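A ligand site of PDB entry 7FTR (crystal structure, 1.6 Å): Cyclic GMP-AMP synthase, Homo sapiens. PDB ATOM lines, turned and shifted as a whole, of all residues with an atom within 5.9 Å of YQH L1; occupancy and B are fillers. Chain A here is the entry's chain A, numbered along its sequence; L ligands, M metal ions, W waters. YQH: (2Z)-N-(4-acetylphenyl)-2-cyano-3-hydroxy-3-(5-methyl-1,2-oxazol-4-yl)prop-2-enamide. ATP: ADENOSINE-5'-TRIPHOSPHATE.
Water W2 lies within hydrogen-bond range of O6 of YQH L1 and O5' of ATP L2.
N3 of ATP L2 sits close to NH1 of Arg 216, at 3.3 Å.
A nitrogen (N14) of YQH L1 lies within hydrogen-bond range of the side-chain hydroxyl (OG) of Ser 218 (2.7 Å).
The side-chain hydroxyl (OG1) of Thr 51 is in hydrogen-bond range of a nitrogen (N9) of YQH L1 (2.9 Å).
O13 of YQH L1 lies within hydrogen-bond range of NH2 of Arg 216 (2.8 Å).
The side-chain hydroxyl of Ser 220 sits at hydrogen-bond distance from an oxygen (O2') of ATP L2 (2.8 Å).
The backbone carbonyl oxygen of Val 68 sits close to an oxygen (O7) of YQH L1 (3.5 Å).
Asp 67 touches YQH L1 (OD1 to C8, 3.6 Å).
Met 69 touches YQH L1.
Ser 145 touches YQH L1.
Pro 146 touches YQH L1.
O of Asp 159 touches C8 of YQH L1, at 3.3 Å.
Thr 161 touches YQH L1 (OG1 to C8, 3.2 Å).
Val 200 touches YQH L1.
Ser 220 touches YQH L1.
Hydrophobic or aromatic side chains within 4 Å of YQH L1: Met 69, Pro 146 and Val 200.
Of the 20 residues printed, 12 come within 4 Å of YQH L1.
The backbone NH (N) of Val 68 lies within hydrogen-bond range of the backbone carbonyl oxygen (O) of Asp 159 (2.9 Å).
N of Ala 147 lies close to OG of Ser 145 (3.3 Å).
O of Arg 216 is in hydrogen-bond range of N of Val 200.
OG of Ser 218 sits at hydrogen-bond distance from OG of Ser 220.
N of Thr 51 lies within hydrogen-bond range of O of Asp 67, 3.1 Å away.
The backbone carbonyl oxygen (O) of Val 68 sits at hydrogen-bond distance from the backbone NH (N) of Thr 161.
N of Asp 159 lies within hydrogen-bond range of O of Phe 66 (2.8 Å).
An oxygen (O4') of ATP L2 sits close to an oxygen (O6) of YQH L1.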
ATOM      1  N   THR A  51      23.136 -30.492  10.259  1.00  0.00           N
ATOM      2  CA  THR A  51      22.006 -30.398  11.183  1.00  0.00           C
ATOM      3  C   THR A  51      21.511 -28.967  11.399  1.00  0.00           C
ATOM      4  O   THR A  51      22.027 -28.009  10.803  1.00  0.00           O
ATOM      5  CB  THR A  51      22.447 -30.994  12.531  1.00  0.00           C
ATOM      6  OG1 THR A  51      23.569 -30.242  12.981  1.00  0.00           O
ATOM      7  CG2 THR A  51      22.790 -32.470  12.451  1.00  0.00           C
ATOM      8  N   GLY A  52      20.533 -28.819  12.268  1.00  0.00           N
ATOM      9  CA  GLY A  52      20.060 -27.485  12.612  1.00  0.00           C
ATOM     10  C   GLY A  52      19.121 -26.890  11.598  1.00  0.00           C
ATOM     11  O   GLY A  52      18.685 -27.562  10.651  1.00  0.00           O
ATOM     12  N   PHE A  66      25.027 -22.059  10.269  1.00  0.00           N
ATOM     13  CA  PHE A  66      24.976 -23.452   9.846  1.00  0.00           C
ATOM     14  C   PHE A  66      25.504 -24.260  11.005  1.00  0.00           C
ATOM     15  O   PHE A  66      26.451 -23.851  11.688  1.00  0.00           O
ATOM     16  CB  PHE A  66      25.914 -23.654   8.649  1.00  0.00           C
ATOM     17  CG  PHE A  66      25.458 -22.979   7.370  1.00  0.00           C
ATOM     18  CD1 PHE A  66      25.561 -21.597   7.228  1.00  0.00           C
ATOM     19  CD2 PHE A  66      24.912 -23.723   6.331  1.00  0.00           C
ATOM     20  CE1 PHE A  66      25.103 -20.966   6.072  1.00  0.00           C
ATOM     21  CE2 PHE A  66      24.497 -23.095   5.151  1.00  0.00           C
ATOM     22  CZ  PHE A  66      24.564 -21.719   5.046  1.00  0.00           C
ATOM     23  N   ASP A  67      24.888 -25.410  11.210  1.00  0.00           N
ATOM     24  CA  ASP A  67      25.280 -26.330  12.261  1.00  0.00           C
ATOM     25  C   ASP A  67      25.675 -27.624  11.613  1.00  0.00           C
ATOM     26  O   ASP A  67      25.020 -28.112  10.675  1.00  0.00           O
ATOM     27  CB  ASP A  67      24.146 -26.515  13.261  1.00  0.00           C
ATOM     28  CG  ASP A  67      23.702 -25.190  13.850  1.00  0.00           C
ATOM     29  OD1 ASP A  67      24.410 -24.679  14.753  1.00  0.00           O
ATOM     30  OD2 ASP A  67      22.598 -24.679  13.423  1.00  0.00           O
ATOM     31  N   VAL A  68      26.784 -28.169  12.104  1.00  0.00           N
ATOM     32  CA  VAL A  68      27.310 -29.412  11.607  1.00  0.00           C
ATOM     33  C   VAL A  68      27.851 -30.269  12.770  1.00  0.00           C
ATOM     34  O   VAL A  68      28.403 -29.737  13.745  1.00  0.00           O
ATOM     35  CB  VAL A  68      28.378 -29.017  10.549  1.00  0.00           C
ATOM     36  CG1 VAL A  68      29.615 -29.888  10.600  1.00  0.00           C
ATOM     37  CG2 VAL A  68      27.792 -28.936   9.140  1.00  0.00           C
ATOM     38  N   MET A  69      27.665 -31.588  12.664  1.00  0.00           N
ATOM     39  CA  MET A  69      28.206 -32.552  13.610  1.00  0.00           C
ATOM     40  C   MET A  69      29.356 -33.259  12.931  1.00  0.00           C
ATOM     41  O   MET A  69      29.210 -33.703  11.781  1.00  0.00           O
ATOM     42  CB  MET A  69      27.183 -33.619  14.048  1.00  0.00           C
ATOM     43  CG  MET A  69      25.871 -33.071  14.564  1.00  0.00           C
ATOM     44  SD  MET A  69      24.984 -34.338  15.515  1.00  0.00           S
ATOM     45  CE  MET A  69      24.040 -35.014  14.352  1.00  0.00           C
ATOM     46  N   GLY A 143      31.417 -21.202  27.547  1.00  0.00           N
ATOM     47  CA  GLY A 143      31.304 -22.083  28.706  1.00  0.00           C
ATOM     48  C   GLY A 143      30.173 -23.074  28.574  1.00  0.00           C
ATOM     49  O   GLY A 143      29.050 -22.717  28.203  1.00  0.00           O
ATOM     50  N   SER A 145      28.887 -25.050  26.365  1.00  0.00           N
ATOM     51  CA  SER A 145      28.607 -25.262  24.934  1.00  0.00           C
ATOM     52  C   SER A 145      29.529 -26.254  24.226  1.00  0.00           C
ATOM     53  O   SER A 145      30.751 -26.137  24.326  1.00  0.00           O
ATOM     54  CB  SER A 145      28.585 -23.939  24.154  1.00  0.00           C
ATOM     55  OG  SER A 145      28.370 -24.172  22.767  1.00  0.00           O
ATOM     56  N   PRO A 146      28.951 -27.215  23.479  1.00  0.00           N
ATOM     57  CA  PRO A 146      29.791 -28.195  22.775  1.00  0.00           C
ATOM     58  C   PRO A 146      30.365 -27.664  21.461  1.00  0.00           C
ATOM     59  O   PRO A 146      31.250 -28.296  20.876  1.00  0.00           O
ATOM     60  CB  PRO A 146      28.823 -29.358  22.550  1.00  0.00           C
ATOM     61  CG  PRO A 146      27.496 -28.681  22.320  1.00  0.00           C
ATOM     62  CD  PRO A 146      27.506 -27.476  23.248  1.00  0.00           C
ATOM     63  N   ALA A 147      29.858 -26.504  20.997  1.00  0.00           N
ATOM     64  CA  ALA A 147      30.200 -25.903  19.712  1.00  0.00           C
ATOM     65  C   ALA A 147      31.534 -25.185  19.644  1.00  0.00           C
ATOM     66  O   ALA A 147      31.962 -24.530  20.598  1.00  0.00           O
ATOM     67  CB  ALA A 147      29.092 -24.960  19.273  1.00  0.00           C
ATOM     68  N   ASP A 159      28.720 -23.576  13.347  1.00  0.00           N
ATOM     69  CA  ASP A 159      28.897 -24.255  14.620  1.00  0.00           C
ATOM     70  C   ASP A 159      29.221 -25.688  14.336  1.00  0.00           C
ATOM     71  O   ASP A 159      28.423 -26.402  13.703  1.00  0.00           O
ATOM     72  CB  ASP A 159      27.638 -24.165  15.515  1.00  0.00           C
ATOM     73  CG  ASP A 159      27.355 -22.835  16.140  1.00  0.00           C
ATOM     74  OD1 ASP A 159      28.281 -21.992  16.205  1.00  0.00           O
ATOM     75  OD2 ASP A 159      26.229 -22.642  16.614  1.00  0.00           O
ATOM     76  N   ILE A 160      30.391 -26.113  14.758  1.00  0.00           N
ATOM     77  CA  ILE A 160      30.851 -27.469  14.551  1.00  0.00           C
ATOM     78  C   ILE A 160      30.883 -28.150  15.903  1.00  0.00           C
ATOM     79  O   ILE A 160      31.596 -27.709  16.809  1.00  0.00           O
ATOM     80  CB  ILE A 160      32.276 -27.487  13.924  1.00  0.00           C
ATOM     81  CG1 ILE A 160      32.350 -26.634  12.651  1.00  0.00           C
ATOM     82  CG2 ILE A 160      32.699 -28.941  13.659  1.00  0.00           C
ATOM     83  CD1 ILE A 160      33.775 -26.301  12.220  1.00  0.00           C
ATOM     84  N   THR A 161      30.169 -29.257  16.028  1.00  0.00           N
ATOM     85  CA  THR A 161      30.261 -29.987  17.285  1.00  0.00           C
ATOM     86  C   THR A 161      30.785 -31.377  16.999  1.00  0.00           C
ATOM     87  O   THR A 161      30.388 -32.007  16.023  1.00  0.00           O
ATOM     88  CB  THR A 161      28.906 -30.052  18.009  1.00  0.00           C
ATOM     89  OG1 THR A 161      28.429 -28.717  18.204  1.00  0.00           O
ATOM     90  CG2 THR A 161      29.022 -30.712  19.356  1.00  0.00           C
ATOM     91  N   VAL A 200      27.447 -35.271  22.599  1.00  0.00           N
ATOM     92  CA  VAL A 200      28.190 -34.050  22.325  1.00  0.00           C
ATOM     93  C   VAL A 200      28.886 -33.555  23.618  1.00  0.00           C
ATOM     94  O   VAL A 200      28.337 -33.745  24.715  1.00  0.00           O
ATOM     95  CB  VAL A 200      27.330 -32.968  21.644  1.00  0.00           C
ATOM     96  CG1 VAL A 200      26.788 -33.460  20.283  1.00  0.00           C
ATOM     97  CG2 VAL A 200      26.196 -32.496  22.564  1.00  0.00           C
ATOM     98  N   LYS A 202      28.812 -31.203  25.674  1.00  0.00           N
ATOM     99  CA  LYS A 202      28.094 -30.155  26.385  1.00  0.00           C
ATOM    100  C   LYS A 202      28.106 -30.687  27.804  1.00  0.00           C
ATOM    101  O   LYS A 202      27.676 -31.825  28.029  1.00  0.00           O
ATOM    102  CB  LYS A 202      26.649 -30.005  25.883  1.00  0.00           C
ATOM    103  CG  LYS A 202      26.006 -28.681  26.320  1.00  0.00           C
ATOM    104  CD  LYS A 202      25.118 -28.821  27.516  1.00  0.00           C
ATOM    105  CE  LYS A 202      24.759 -27.494  28.139  1.00  0.00           C
ATOM    106  NZ  LYS A 202      25.870 -26.975  28.980  1.00  0.00           N
ATOM    107  N   ARG A 216      26.547 -34.883  26.621  1.00  0.00           N
ATOM    108  CA  ARG A 216      25.079 -34.851  26.588  1.00  0.00           C
ATOM    109  C   ARG A 216      24.530 -35.515  25.340  1.00  0.00           C
ATOM    110  O   ARG A 216      25.142 -35.410  24.267  1.00  0.00           O
ATOM    111  CB  ARG A 216      24.529 -33.409  26.688  1.00  0.00           C
ATOM    112  CG  ARG A 216      23.031 -33.382  27.085  1.00  0.00           C
ATOM    113  CD  ARG A 216      22.280 -32.193  26.558  1.00  0.00           C
ATOM    114  NE  ARG A 216      22.208 -32.317  25.098  1.00  0.00           N
ATOM    115  CZ  ARG A 216      22.623 -31.398  24.238  1.00  0.00           C
ATOM    116  NH1 ARG A 216      22.619 -31.660  22.937  1.00  0.00           N
ATOM    117  NH2 ARG A 216      23.017 -30.199  24.664  1.00  0.00           N
ATOM    118  N   LEU A 217      23.349 -36.164  25.476  1.00  0.00           N
ATOM    119  CA  LEU A 217      22.677 -36.800  24.347  1.00  0.00           C
ATOM    120  C   LEU A 217      22.253 -35.765  23.322  1.00  0.00           C
ATOM    121  O   LEU A 217      21.793 -34.673  23.675  1.00  0.00           O
ATOM    122  CB  LEU A 217      21.456 -37.658  24.761  1.00  0.00           C
ATOM    123  CG  LEU A 217      21.725 -38.920  25.603  1.00  0.00           C
ATOM    124  CD1 LEU A 217      20.418 -39.616  25.990  1.00  0.00           C
ATOM    125  CD2 LEU A 217      22.597 -39.907  24.856  1.00  0.00           C
ATOM    126  N   SER A 218      22.439 -36.114  22.055  1.00  0.00           N
ATOM    127  CA  SER A 218      22.005 -35.280  20.942  1.00  0.00           C
ATOM    128  C   SER A 218      21.198 -36.111  19.937  1.00  0.00           C
ATOM    129  O   SER A 218      21.620 -37.199  19.523  1.00  0.00           O
ATOM    130  CB  SER A 218      23.190 -34.630  20.221  1.00  0.00           C
ATOM    131  OG  SER A 218      22.724 -33.938  19.065  1.00  0.00           O
ATOM    132  N   PHE A 219      20.076 -35.562  19.531  1.00  0.00           N
ATOM    133  CA  PHE A 219      19.207 -36.219  18.555  1.00  0.00           C
ATOM    134  C   PHE A 219      18.962 -35.291  17.381  1.00  0.00           C
ATOM    135  O   PHE A 219      17.944 -35.414  16.711  1.00  0.00           O
ATOM    136  CB  PHE A 219      17.908 -36.698  19.217  1.00  0.00           C
ATOM    137  CG  PHE A 219      18.157 -37.833  20.186  1.00  0.00           C
ATOM    138  CD1 PHE A 219      18.303 -39.137  19.725  1.00  0.00           C
ATOM    139  CD2 PHE A 219      18.279 -37.591  21.558  1.00  0.00           C
ATOM    140  CE1 PHE A 219      18.581 -40.177  20.615  1.00  0.00           C
ATOM    141  CE2 PHE A 219      18.544 -38.636  22.451  1.00  0.00           C
ATOM    142  CZ  PHE A 219      18.687 -39.922  21.973  1.00  0.00           C
ATOM    143  N   SER A 220      19.938 -34.416  17.079  1.00  0.00           N
ATOM    144  CA  SER A 220      19.850 -33.436  15.968  1.00  0.00           C
ATOM    145  C   SER A 220      19.502 -34.091  14.624  1.00  0.00           C
ATOM    146  O   SER A 220      18.767 -33.500  13.816  1.00  0.00           O
ATOM    147  CB  SER A 220      21.188 -32.715  15.825  1.00  0.00           C
ATOM    148  OG  SER A 220      21.510 -32.009  17.005  1.00  0.00           O
HETATM  149  C10 YQH L   1      23.957 -28.425  21.265  1.00  0.00           C
HETATM  150  C11 YQH L   1      23.889 -30.418  19.809  1.00  0.00           C
HETATM  151  C15 YQH L   1      24.115 -26.274  22.571  1.00  0.00           C
HETATM  152  C16 YQH L   1      23.362 -26.597  23.701  1.00  0.00           C
HETATM  153  C17 YQH L   1      24.812 -25.063  22.550  1.00  0.00           C
HETATM  154  C18 YQH L   1      23.335 -25.747  24.800  1.00  0.00           C
HETATM  155  C19 YQH L   1      24.776 -24.209  23.648  1.00  0.00           C
HETATM  156  C20 YQH L   1      24.048 -24.548  24.792  1.00  0.00           C
HETATM  157  C21 YQH L   1      23.999 -23.634  25.976  1.00  0.00           C
HETATM  158  C22 YQH L   1      24.777 -22.352  25.955  1.00  0.00           C
HETATM  159  C1  YQH L   1      24.795 -28.922  17.457  1.00  0.00           C
HETATM  160  C2  YQH L   1      24.622 -28.363  18.809  1.00  0.00           C
HETATM  161  C3  YQH L   1      25.519 -28.471  16.391  1.00  0.00           C
HETATM  162  C4  YQH L   1      24.151 -30.079  16.965  1.00  0.00           C
HETATM  163  C5  YQH L   1      24.161 -29.013  19.930  1.00  0.00           C
HETATM  164  O6  YQH L   1      24.867 -27.064  18.863  1.00  0.00           O
HETATM  165  O7  YQH L   1      25.330 -29.293  15.345  1.00  0.00           O
HETATM  166  C8  YQH L   1      26.417 -27.320  16.159  1.00  0.00           C
HETATM  167  N9  YQH L   1      24.451 -30.326  15.725  1.00  0.00           N
HETATM  168  N12 YQH L   1      24.192 -27.087  21.413  1.00  0.00           N
HETATM  169  O13 YQH L   1      23.548 -29.128  22.187  1.00  0.00           O
HETATM  170  N14 YQH L   1      23.702 -31.537  19.772  1.00  0.00           N
HETATM  171  O23 YQH L   1      23.337 -23.931  26.972  1.00  0.00           O
HETATM  172  PG  ATP L   2      18.795 -21.368  14.706  1.00  0.00           P
HETATM  173  O1G ATP L   2      20.253 -21.602  14.385  1.00  0.00           O
HETATM  174  O2G ATP L   2      18.463 -20.519  15.898  1.00  0.00           O
HETATM  175  O3G ATP L   2      17.969 -20.882  13.561  1.00  0.00           O
HETATM  176  PB  ATP L   2      18.950 -24.198  15.257  1.00  0.00           P
HETATM  177  O1B ATP L   2      17.995 -25.340  15.395  1.00  0.00           O
HETATM  178  O2B ATP L   2      19.991 -24.509  14.183  1.00  0.00           O
HETATM  179  O3B ATP L   2      18.219 -22.821  14.971  1.00  0.00           O
HETATM  180  PA  ATP L   2      21.211 -24.111  17.163  1.00  0.00           P
HETATM  181  O1A ATP L   2      21.316 -23.269  18.379  1.00  0.00           O
HETATM  182  O2A ATP L   2      21.984 -23.549  15.989  1.00  0.00           O
HETATM  183  O3A ATP L   2      19.705 -24.009  16.651  1.00  0.00           O
HETATM  184  O5' ATP L   2      21.538 -25.626  17.353  1.00  0.00           O
HETATM  185  C5' ATP L   2      21.690 -26.567  16.296  1.00  0.00           C
HETATM  186  C4' ATP L   2      21.063 -27.852  16.762  1.00  0.00           C
HETATM  187  O4' ATP L   2      21.699 -28.266  17.985  1.00  0.00           O
HETATM  188  C3' ATP L   2      19.585 -27.776  17.129  1.00  0.00           C
HETATM  189  O3' ATP L   2      18.750 -27.840  15.975  1.00  0.00           O
HETATM  190  C2' ATP L   2      19.428 -28.993  18.027  1.00  0.00           C
HETATM  191  O2' ATP L   2      19.366 -30.177  17.245  1.00  0.00           O
HETATM  192  C1' ATP L   2      20.776 -28.979  18.789  1.00  0.00           C
HETATM  193  N9  ATP L   2      20.704 -28.331  20.090  1.00  0.00           N
HETATM  194  C8  ATP L   2      20.866 -26.998  20.385  1.00  0.00           C
HETATM  195  N7  ATP L   2      20.632 -26.692  21.640  1.00  0.00           N
HETATM  196  C5  ATP L   2      20.317 -27.909  22.223  1.00  0.00           C
HETATM  197  C6  ATP L   2      19.999 -28.278  23.541  1.00  0.00           C
HETATM  198  N6  ATP L   2      19.910 -27.403  24.552  1.00  0.00           N
HETATM  199  N1  ATP L   2      19.712 -29.572  23.776  1.00  0.00           N
HETATM  200  C2  ATP L   2      19.748 -30.447  22.771  1.00  0.00           C
HETATM  201  N3  ATP L   2      20.060 -30.224  21.483  1.00  0.00           N
HETATM  202  C4  ATP L   2      20.347 -28.929  21.279  1.00  0.00           C
HETATM  203 MG    MG M   1      24.202 -23.252  16.294  1.00  0.00          MG
HETATM  204  O   HOH W   1      23.149 -23.096  20.295  1.00  0.00           O
HETATM  205  O   HOH W   2      24.681 -24.736  17.726  1.00  0.00           O
